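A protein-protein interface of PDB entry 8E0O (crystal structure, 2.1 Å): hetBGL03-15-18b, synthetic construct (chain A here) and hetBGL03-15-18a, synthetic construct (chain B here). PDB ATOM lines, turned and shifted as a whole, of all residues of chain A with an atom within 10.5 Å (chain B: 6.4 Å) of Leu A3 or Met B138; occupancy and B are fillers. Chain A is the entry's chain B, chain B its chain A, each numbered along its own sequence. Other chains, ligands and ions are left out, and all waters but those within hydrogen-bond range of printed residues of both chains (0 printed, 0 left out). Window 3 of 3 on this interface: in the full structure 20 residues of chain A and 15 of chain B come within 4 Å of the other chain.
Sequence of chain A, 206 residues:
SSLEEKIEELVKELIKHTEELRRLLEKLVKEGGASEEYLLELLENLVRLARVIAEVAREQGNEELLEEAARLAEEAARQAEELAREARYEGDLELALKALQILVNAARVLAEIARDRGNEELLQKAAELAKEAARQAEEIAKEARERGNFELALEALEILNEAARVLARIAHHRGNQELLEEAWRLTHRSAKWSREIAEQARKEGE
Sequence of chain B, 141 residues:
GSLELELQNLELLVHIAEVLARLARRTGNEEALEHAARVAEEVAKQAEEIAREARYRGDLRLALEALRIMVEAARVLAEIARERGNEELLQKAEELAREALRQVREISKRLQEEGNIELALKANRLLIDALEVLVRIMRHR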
ATOM      1  N   SER A   1     -12.560   9.961  -2.854  1.00  0.00           N
ATOM      2  CA  SER A   1     -12.905  11.035  -3.779  1.00  0.00           C
ATOM      3  C   SER A   1     -12.074  12.283  -3.498  1.00  0.00           C
ATOM      4  O   SER A   1     -10.896  12.344  -3.851  1.00  0.00           O
ATOM      5  CB  SER A   1     -14.396  11.362  -3.691  1.00  0.00           C
ATOM      6  N   SER A   2     -12.695  13.278  -2.859  1.00  0.00           N
ATOM      7  CA  SER A   2     -11.969  14.496  -2.516  1.00  0.00           C
ATOM      8  C   SER A   2     -10.869  14.225  -1.499  1.00  0.00           C
ATOM      9  O   SER A   2      -9.809  14.860  -1.551  1.00  0.00           O
ATOM     10  CB  SER A   2     -12.935  15.556  -1.986  1.00  0.00           C
ATOM     11  OG  SER A   2     -12.245  16.743  -1.638  1.00  0.00           O
ATOM     12  N   LEU A   3     -11.100  13.296  -0.568  1.00  0.00           N
ATOM     13  CA  LEU A   3     -10.025  12.867   0.322  1.00  0.00           C
ATOM     14  C   LEU A   3      -8.926  12.161  -0.459  1.00  0.00           C
ATOM     15  O   LEU A   3      -7.736  12.341  -0.172  1.00  0.00           O
ATOM     16  CB  LEU A   3     -10.579  11.956   1.418  1.00  0.00           C
ATOM     17  CG  LEU A   3      -9.555  11.366   2.390  1.00  0.00           C
ATOM     18  CD1 LEU A   3      -9.537  12.143   3.698  1.00  0.00           C
ATOM     19  CD2 LEU A   3      -9.837   9.892   2.641  1.00  0.00           C
ATOM     20  N   GLU A   4      -9.307  11.352  -1.451  1.00  0.00           N
ATOM     21  CA  GLU A   4      -8.316  10.746  -2.333  1.00  0.00           C
ATOM     22  C   GLU A   4      -7.598  11.806  -3.157  1.00  0.00           C
ATOM     23  O   GLU A   4      -6.398  11.684  -3.434  1.00  0.00           O
ATOM     24  CB  GLU A   4      -8.986   9.721  -3.246  1.00  0.00           C
ATOM     25  N   GLU A   5      -8.319  12.855  -3.559  1.00  0.00           N
ATOM     26  CA  GLU A   5      -7.696  13.946  -4.300  1.00  0.00           C
ATOM     27  C   GLU A   5      -6.700  14.709  -3.436  1.00  0.00           C
ATOM     28  O   GLU A   5      -5.675  15.181  -3.942  1.00  0.00           O
ATOM     29  CB  GLU A   5      -8.769  14.890  -4.842  1.00  0.00           C
ATOM     30  CG  GLU A   5      -9.546  14.333  -6.025  1.00  0.00           C
ATOM     31  CD  GLU A   5     -10.235  15.414  -6.835  1.00  0.00           C
ATOM     32  OE1 GLU A   5     -10.083  15.418  -8.074  1.00  0.00           O
ATOM     33  OE2 GLU A   5     -10.930  16.258  -6.231  1.00  0.00           O
ATOM     34  N   LYS A   6      -6.980  14.841  -2.137  1.00  0.00           N
ATOM     35  CA  LYS A   6      -6.031  15.488  -1.239  1.00  0.00           C
ATOM     36  C   LYS A   6      -4.799  14.619  -1.023  1.00  0.00           C
ATOM     37  O   LYS A   6      -3.679  15.133  -0.925  1.00  0.00           O
ATOM     38  CB  LYS A   6      -6.703  15.805   0.097  1.00  0.00           C
ATOM     39  CG  LYS A   6      -7.159  17.248   0.241  1.00  0.00           C
ATOM     40  CD  LYS A   6      -8.628  17.322   0.622  1.00  0.00           C
ATOM     41  CE  LYS A   6      -8.797  17.571   2.112  1.00  0.00           C
ATOM     42  NZ  LYS A   6     -10.220  17.814   2.479  1.00  0.00           N
ATOM     43  N   ILE A   7      -4.987  13.300  -0.944  1.00  0.00           N
ATOM     44  CA  ILE A   7      -3.856  12.396  -0.766  1.00  0.00           C
ATOM     45  C   ILE A   7      -2.974  12.395  -2.009  1.00  0.00           C
ATOM     46  O   ILE A   7      -1.741  12.411  -1.911  1.00  0.00           O
ATOM     47  CB  ILE A   7      -4.355  10.981  -0.417  1.00  0.00           C
ATOM     48  CG1 ILE A   7      -4.951  10.958   0.991  1.00  0.00           C
ATOM     49  CG2 ILE A   7      -3.228   9.964  -0.534  1.00  0.00           C
ATOM     50  CD1 ILE A   7      -5.580   9.635   1.368  1.00  0.00           C
ATOM     51  N   GLU A   8      -3.587  12.381  -3.195  1.00  0.00           N
ATOM     52  CA  GLU A   8      -2.810  12.436  -4.428  1.00  0.00           C
ATOM     53  C   GLU A   8      -2.063  13.757  -4.559  1.00  0.00           C
ATOM     54  O   GLU A   8      -0.958  13.792  -5.114  1.00  0.00           O
ATOM     55  CB  GLU A   8      -3.722  12.218  -5.636  1.00  0.00           C
ATOM     56  N   GLU A   9      -2.643  14.848  -4.056  1.00  0.00           N
ATOM     57  CA  GLU A   9      -1.949  16.131  -4.082  1.00  0.00           C
ATOM     58  C   GLU A   9      -0.759  16.132  -3.128  1.00  0.00           C
ATOM     59  O   GLU A   9       0.283  16.729  -3.424  1.00  0.00           O
ATOM     60  CB  GLU A   9      -2.924  17.259  -3.741  1.00  0.00           C
ATOM     61  CG  GLU A   9      -2.267  18.572  -3.350  1.00  0.00           C
ATOM     62  CD  GLU A   9      -3.129  19.776  -3.683  1.00  0.00           C
ATOM     63  OE1 GLU A   9      -4.325  19.774  -3.320  1.00  0.00           O
ATOM     64  OE2 GLU A   9      -2.610  20.724  -4.308  1.00  0.00           O
ATOM     65  N   LEU A  10      -0.892  15.455  -1.984  1.00  0.00           N
ATOM     66  CA  LEU A  10       0.218  15.371  -1.040  1.00  0.00           C
ATOM     67  C   LEU A  10       1.357  14.526  -1.598  1.00  0.00           C
ATOM     68  O   LEU A  10       2.531  14.890  -1.459  1.00  0.00           O
ATOM     69  CB  LEU A  10      -0.269  14.799   0.292  1.00  0.00           C
ATOM     70  CG  LEU A  10      -1.038  15.742   1.218  1.00  0.00           C
ATOM     71  CD1 LEU A  10      -1.745  14.954   2.310  1.00  0.00           C
ATOM     72  CD2 LEU A  10      -0.105  16.778   1.824  1.00  0.00           C
ATOM     73  N   VAL A  11       1.032  13.394  -2.226  1.00  0.00           N
ATOM     74  CA  VAL A  11       2.067  12.539  -2.801  1.00  0.00           C
ATOM     75  C   VAL A  11       2.755  13.243  -3.964  1.00  0.00           C
ATOM     76  O   VAL A  11       3.975  13.136  -4.138  1.00  0.00           O
ATOM     77  CB  VAL A  11       1.464  11.188  -3.227  1.00  0.00           C
ATOM     78  CG1 VAL A  11       2.509  10.329  -3.926  1.00  0.00           C
ATOM     79  CG2 VAL A  11       0.894  10.460  -2.018  1.00  0.00           C
ATOM     80  N   GLU A  55       1.987   2.199  -2.228  1.00  0.00           N
ATOM     81  CA  GLU A  55       0.976   1.910  -1.216  1.00  0.00           C
ATOM     82  C   GLU A  55      -0.215   2.851  -1.346  1.00  0.00           C
ATOM     83  O   GLU A  55      -1.360   2.449  -1.109  1.00  0.00           O
ATOM     84  CB  GLU A  55       1.590   2.004   0.181  1.00  0.00           C
ATOM     85  CG  GLU A  55       0.691   1.486   1.291  1.00  0.00           C
ATOM     86  CD  GLU A  55       0.844   2.272   2.578  1.00  0.00           C
ATOM     87  OE1 GLU A  55       1.917   2.174   3.211  1.00  0.00           O
ATOM     88  OE2 GLU A  55      -0.106   2.988   2.955  1.00  0.00           O
ATOM     89  N   VAL A  56       0.034   4.106  -1.723  1.00  0.00           N
ATOM     90  CA  VAL A  56      -1.059   5.047  -1.943  1.00  0.00           C
ATOM     91  C   VAL A  56      -1.827   4.683  -3.207  1.00  0.00           C
ATOM     92  O   VAL A  56      -3.064   4.715  -3.231  1.00  0.00           O
ATOM     93  CB  VAL A  56      -0.517   6.488  -1.998  1.00  0.00           C
ATOM     94  CG1 VAL A  56      -1.460   7.392  -2.781  1.00  0.00           C
ATOM     95  CG2 VAL A  56      -0.297   7.026  -0.593  1.00  0.00           C
ATOM     96  N   GLU A  59      -4.445   1.590  -2.966  1.00  0.00           N
ATOM     97  CA  GLU A  59      -5.757   1.810  -2.370  1.00  0.00           C
ATOM     98  C   GLU A  59      -6.646   2.688  -3.241  1.00  0.00           C
ATOM     99  O   GLU A  59      -7.871   2.529  -3.222  1.00  0.00           O
ATOM    100  CB  GLU A  59      -5.606   2.436  -0.982  1.00  0.00           C
ATOM    101  CG  GLU A  59      -6.828   2.277  -0.091  1.00  0.00           C
ATOM    102  N   GLN A  60      -6.060   3.608  -4.004  1.00  0.00           N
ATOM    103  CA  GLN A  60      -6.828   4.509  -4.853  1.00  0.00           C
ATOM    104  C   GLN A  60      -7.051   3.960  -6.255  1.00  0.00           C
ATOM    105  O   GLN A  60      -7.731   4.610  -7.056  1.00  0.00           O
ATOM    106  CB  GLN A  60      -6.134   5.873  -4.947  1.00  0.00           C
ATOM    107  CG  GLN A  60      -5.773   6.510  -3.609  1.00  0.00           C
ATOM    108  CD  GLN A  60      -6.846   6.334  -2.548  1.00  0.00           C
ATOM    109  OE1 GLN A  60      -6.562   5.907  -1.430  1.00  0.00           O
ATOM    110  NE2 GLN A  60      -8.083   6.679  -2.888  1.00  0.00           N
ATOM    111  N   LEU B  90      -8.650  11.634  16.708  1.00  0.00           N
ATOM    112  CA  LEU B  90      -8.094  11.371  15.385  1.00  0.00           C
ATOM    113  C   LEU B  90      -7.730  12.668  14.675  1.00  0.00           C
ATOM    114  O   LEU B  90      -6.697  12.745  13.999  1.00  0.00           O
ATOM    115  CB  LEU B  90      -9.085  10.558  14.552  1.00  0.00           C
ATOM    116  CG  LEU B  90      -8.597  10.095  13.178  1.00  0.00           C
ATOM    117  CD1 LEU B  90      -7.311   9.291  13.309  1.00  0.00           C
ATOM    118  CD2 LEU B  90      -9.672   9.282  12.478  1.00  0.00           C
ATOM    119  N   GLU B  94      -4.082  13.906  13.389  1.00  0.00           N
ATOM    120  CA  GLU B  94      -3.839  14.357  12.023  1.00  0.00           C
ATOM    121  C   GLU B  94      -3.203  15.741  12.003  1.00  0.00           C
ATOM    122  O   GLU B  94      -2.311  16.009  11.191  1.00  0.00           O
ATOM    123  CB  GLU B  94      -5.142  14.357  11.223  1.00  0.00           C
ATOM    124  CG  GLU B  94      -4.942  14.569   9.728  1.00  0.00           C
ATOM    125  CD  GLU B  94      -6.242  14.829   8.991  1.00  0.00           C
ATOM    126  OE1 GLU B  94      -7.205  14.061   9.192  1.00  0.00           O
ATOM    127  OE2 GLU B  94      -6.297  15.800   8.207  1.00  0.00           O
ATOM    128  N   ARG B  98       0.347  16.762  10.474  1.00  0.00           N
ATOM    129  CA  ARG B  98       0.419  17.843   9.496  1.00  0.00           C
ATOM    130  C   ARG B  98       1.401  18.922   9.936  1.00  0.00           C
ATOM    131  O   ARG B  98       2.155  19.455   9.113  1.00  0.00           O
ATOM    132  CB  ARG B  98      -0.967  18.446   9.274  1.00  0.00           C
ATOM    133  CG  ARG B  98      -1.827  17.688   8.282  1.00  0.00           C
ATOM    134  CD  ARG B  98      -3.145  18.410   8.054  1.00  0.00           C
ATOM    135  NE  ARG B  98      -4.040  17.659   7.182  1.00  0.00           N
ATOM    136  CZ  ARG B  98      -3.877  17.527   5.872  1.00  0.00           C
ATOM    137  NH1 ARG B  98      -2.851  18.079   5.243  1.00  0.00           N
ATOM    138  NH2 ARG B  98      -4.766  16.827   5.177  1.00  0.00           N
ATOM    139  N   VAL B 133       2.755   8.455   7.350  1.00  0.00           N
ATOM    140  CA  VAL B 133       1.962   8.479   8.574  1.00  0.00           C
ATOM    141  C   VAL B 133       0.697   9.303   8.370  1.00  0.00           C
ATOM    142  O   VAL B 133      -0.404   8.885   8.747  1.00  0.00           O
ATOM    143  CB  VAL B 133       2.805   9.010   9.747  1.00  0.00           C
ATOM    144  CG1 VAL B 133       1.909   9.473  10.887  1.00  0.00           C
ATOM    145  CG2 VAL B 133       3.778   7.942  10.226  1.00  0.00           C
ATOM    146  N   LEU B 134       0.834  10.482   7.754  1.00  0.00           N
ATOM    147  CA  LEU B 134      -0.322  11.350   7.542  1.00  0.00           C
ATOM    148  C   LEU B 134      -1.357  10.684   6.644  1.00  0.00           C
ATOM    149  O   LEU B 134      -2.558  10.715   6.934  1.00  0.00           O
ATOM    150  CB  LEU B 134       0.128  12.686   6.946  1.00  0.00           C
ATOM    151  CG  LEU B 134      -0.980  13.642   6.491  1.00  0.00           C
ATOM    152  CD1 LEU B 134      -1.949  13.943   7.629  1.00  0.00           C
ATOM    153  CD2 LEU B 134      -0.392  14.929   5.931  1.00  0.00           C
ATOM    154  N   VAL B 135      -0.907  10.076   5.543  1.00  0.00           N
ATOM    155  CA  VAL B 135      -1.835   9.433   4.615  1.00  0.00           C
ATOM    156  C   VAL B 135      -2.579   8.296   5.307  1.00  0.00           C
ATOM    157  O   VAL B 135      -3.790   8.124   5.120  1.00  0.00           O
ATOM    158  CB  VAL B 135      -1.083   8.944   3.363  1.00  0.00           C
ATOM    159  CG1 VAL B 135      -1.897   7.892   2.622  1.00  0.00           C
ATOM    160  CG2 VAL B 135      -0.761  10.115   2.449  1.00  0.00           C
ATOM    161  N   ARG B 136      -1.873   7.513   6.126  1.00  0.00           N
ATOM    162  CA  ARG B 136      -2.527   6.446   6.874  1.00  0.00           C
ATOM    163  C   ARG B 136      -3.555   7.009   7.851  1.00  0.00           C
ATOM    164  O   ARG B 136      -4.627   6.422   8.044  1.00  0.00           O
ATOM    165  CB  ARG B 136      -1.483   5.606   7.611  1.00  0.00           C
ATOM    166  CG  ARG B 136      -2.048   4.740   8.726  1.00  0.00           C
ATOM    167  CD  ARG B 136      -1.028   3.733   9.233  1.00  0.00           C
ATOM    168  NE  ARG B 136       0.015   3.458   8.252  1.00  0.00           N
ATOM    169  CZ  ARG B 136       1.314   3.558   8.492  1.00  0.00           C
ATOM    170  NH1 ARG B 136       1.771   3.938   9.675  1.00  0.00           N
ATOM    171  NH2 ARG B 136       2.178   3.271   7.523  1.00  0.00           N
ATOM    172  N   ILE B 137      -3.249   8.154   8.468  1.00  0.00           N
ATOM    173  CA  ILE B 137      -4.193   8.781   9.390  1.00  0.00           C
ATOM    174  C   ILE B 137      -5.457   9.203   8.652  1.00  0.00           C
ATOM    175  O   ILE B 137      -6.577   9.009   9.141  1.00  0.00           O
ATOM    176  CB  ILE B 137      -3.532   9.977  10.102  1.00  0.00           C
ATOM    177  CG1 ILE B 137      -2.433   9.499  11.051  1.00  0.00           C
ATOM    178  CG2 ILE B 137      -4.568  10.783  10.867  1.00  0.00           C
ATOM    179  CD1 ILE B 137      -1.607  10.623  11.643  1.00  0.00           C
ATOM    180  N   MET B 138      -5.298   9.782   7.461  1.00  0.00           N
ATOM    181  CA  MET B 138      -6.444  10.237   6.685  1.00  0.00           C
ATOM    182  C   MET B 138      -7.296   9.093   6.152  1.00  0.00           C
ATOM    183  O   MET B 138      -8.445   9.327   5.765  1.00  0.00           O
ATOM    184  CB  MET B 138      -5.971  11.104   5.518  1.00  0.00           C
ATOM    185  CG  MET B 138      -5.134  12.301   5.923  1.00  0.00           C
ATOM    186  SD  MET B 138      -4.427  13.119   4.482  1.00  0.00           S
ATOM    187  CE  MET B 138      -5.843  14.036   3.877  1.00  0.00           C
ATOM    188  N   ARG B 139      -6.773   7.867   6.131  1.00  0.00           N
ATOM    189  CA  ARG B 139      -7.461   6.779   5.447  1.00  0.00           C
ATOM    190  C   ARG B 139      -8.350   5.946   6.362  1.00  0.00           C
ATOM    191  O   ARG B 139      -9.354   5.397   5.893  1.00  0.00           O
ATOM    192  CB  ARG B 139      -6.444   5.872   4.752  1.00  0.00           C
ATOM    193  CG  ARG B 139      -5.938   6.445   3.439  1.00  0.00           C
ATOM    194  CD  ARG B 139      -5.061   5.459   2.695  1.00  0.00           C
ATOM    195  NE  ARG B 139      -5.023   5.747   1.266  1.00  0.00           N
ATOM    196  CZ  ARG B 139      -4.132   5.242   0.425  1.00  0.00           C
ATOM    197  NH1 ARG B 139      -3.183   4.417   0.834  1.00  0.00           N
ATOM    198  NH2 ARG B 139      -4.195   5.575  -0.862  1.00  0.00           N
ATOM    199  N   HIS B 140      -8.021   5.826   7.652  1.00  0.00           N
ATOM    200  CA  HIS B 140      -8.869   5.084   8.577  1.00  0.00           C
ATOM    201  C   HIS B 140      -9.880   5.977   9.291  1.00  0.00           C
ATOM    202  O   HIS B 140     -10.233   5.712  10.449  1.00  0.00           O
ATOM    203  CB  HIS B 140      -8.019   4.306   9.586  1.00  0.00           C
ATOM    204  CG  HIS B 140      -7.002   5.135  10.308  1.00  0.00           C
ATOM    205  ND1 HIS B 140      -5.781   4.632  10.699  1.00  0.00           N
ATOM    206  CD2 HIS B 140      -7.032   6.422  10.731  1.00  0.00           C
ATOM    207  CE1 HIS B 140      -5.095   5.575  11.321  1.00  0.00           C
ATOM    208  NE2 HIS B 140      -5.833   6.670  11.354  1.00  0.00           N
ATOM    209  N   ARG B 141     -10.355   7.026   8.625  1.00  0.00           N
ATOM    210  CA  ARG B 141     -11.407   7.880   9.163  1.00  0.00           C
ATOM    211  C   ARG B 141     -12.711   7.624   8.416  1.00  0.00           C
ATOM    212  O   ARG B 141     -12.703   7.250   7.245  1.00  0.00           O
ATOM    213  CB  ARG B 141     -11.011   9.356   9.065  1.00  0.00           C
ATOM    214  CG  ARG B 141     -12.159  10.342   9.271  1.00  0.00           C
ATOM    215  CD  ARG B 141     -12.870  10.136  10.604  1.00  0.00           C
ATOM    216  NE  ARG B 141     -14.100  10.916  10.692  1.00  0.00           N
ATOM    217  CZ  ARG B 141     -15.277  10.508  10.238  1.00  0.00           C
ATOM    218  NH1 ARG B 141     -16.364  11.254  10.362  1.00  0.00           N
ATOM    219  NH2 ARG B 141     -15.367   9.325   9.638  1.00  0.00           N
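The guanidinium group (NH2) of Arg B98 lies close to the side-chain sulfur (SD) of Met B138.
Among the printed residues, pairs that only touch across the chains: Glu A59 with Arg B139 (3.4 Å), Leu A3 with Met B138 (3.5 Å), Val A56 with Val B135 (3.7 Å), Ile A7 with Arg B139 (3.8 Å), Leu A10 with Leu B134 (3.9 Å), Ile A7 with Val B135 (3.9 Å) and Leu A10 with Met B138 (3.9 Å).
Hydrophobic or aromatic side chains of chain B that line the printed part of chain A: Leu B134, Val B135 and Met B138. Hydrophobic or aromatic side chains of chain A within 4 Å of the printed part of chain B: Leu A3, Ile A7, Leu A10 and Val A56. Among the printed residues, no Asp or Glu carboxylate lies within 4 Å of a Lys or Arg side-chain nitrogen of the other chain.
The guanidinium group (NH1) of Arg B139 sits at hydrogen-bond distance from the backbone carbonyl oxygen (O) of Glu A55 (3.3 Å). NH2 of Arg B139 sits at hydrogen-bond distance from O of Val A56 (2.8 Å). The guanidinium group (NH2) of Arg B139 is in hydrogen-bond range of the side-chain amide oxygen (OE1) of Gln A60 (2.5 Å).
Of chain B, only Met B138 (3.5 Å) comes within 4 Å of Leu A3. Of the printed residues of chain B, Val A56 touches Val B135 (3.7 Å) and Arg B139 (2.8 Å). Met B138 touches just these residues of chain A: Leu A3 (3.5 Å) and Leu A10 (3.9 Å). Printed residues of chain A within 4 Å of Arg B139: Ile A7 (3.8 Å), Glu A55 (3.3 Å), Val A56 (2.8 Å), Glu A59 (3.4 Å) and Gln A60 (2.5 Å). No residue of chain A comes within 4 Å of His B140. The nearest residue of chain B that does not touch Leu A3 is Arg B139 (4.8 Å). The nearest residue of chain A that does not touch Met B138 is Ile A7 (4.1 Å). The nearest printed residue of chain B that does not touch Leu A10 is Arg B98 (4.4 Å).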
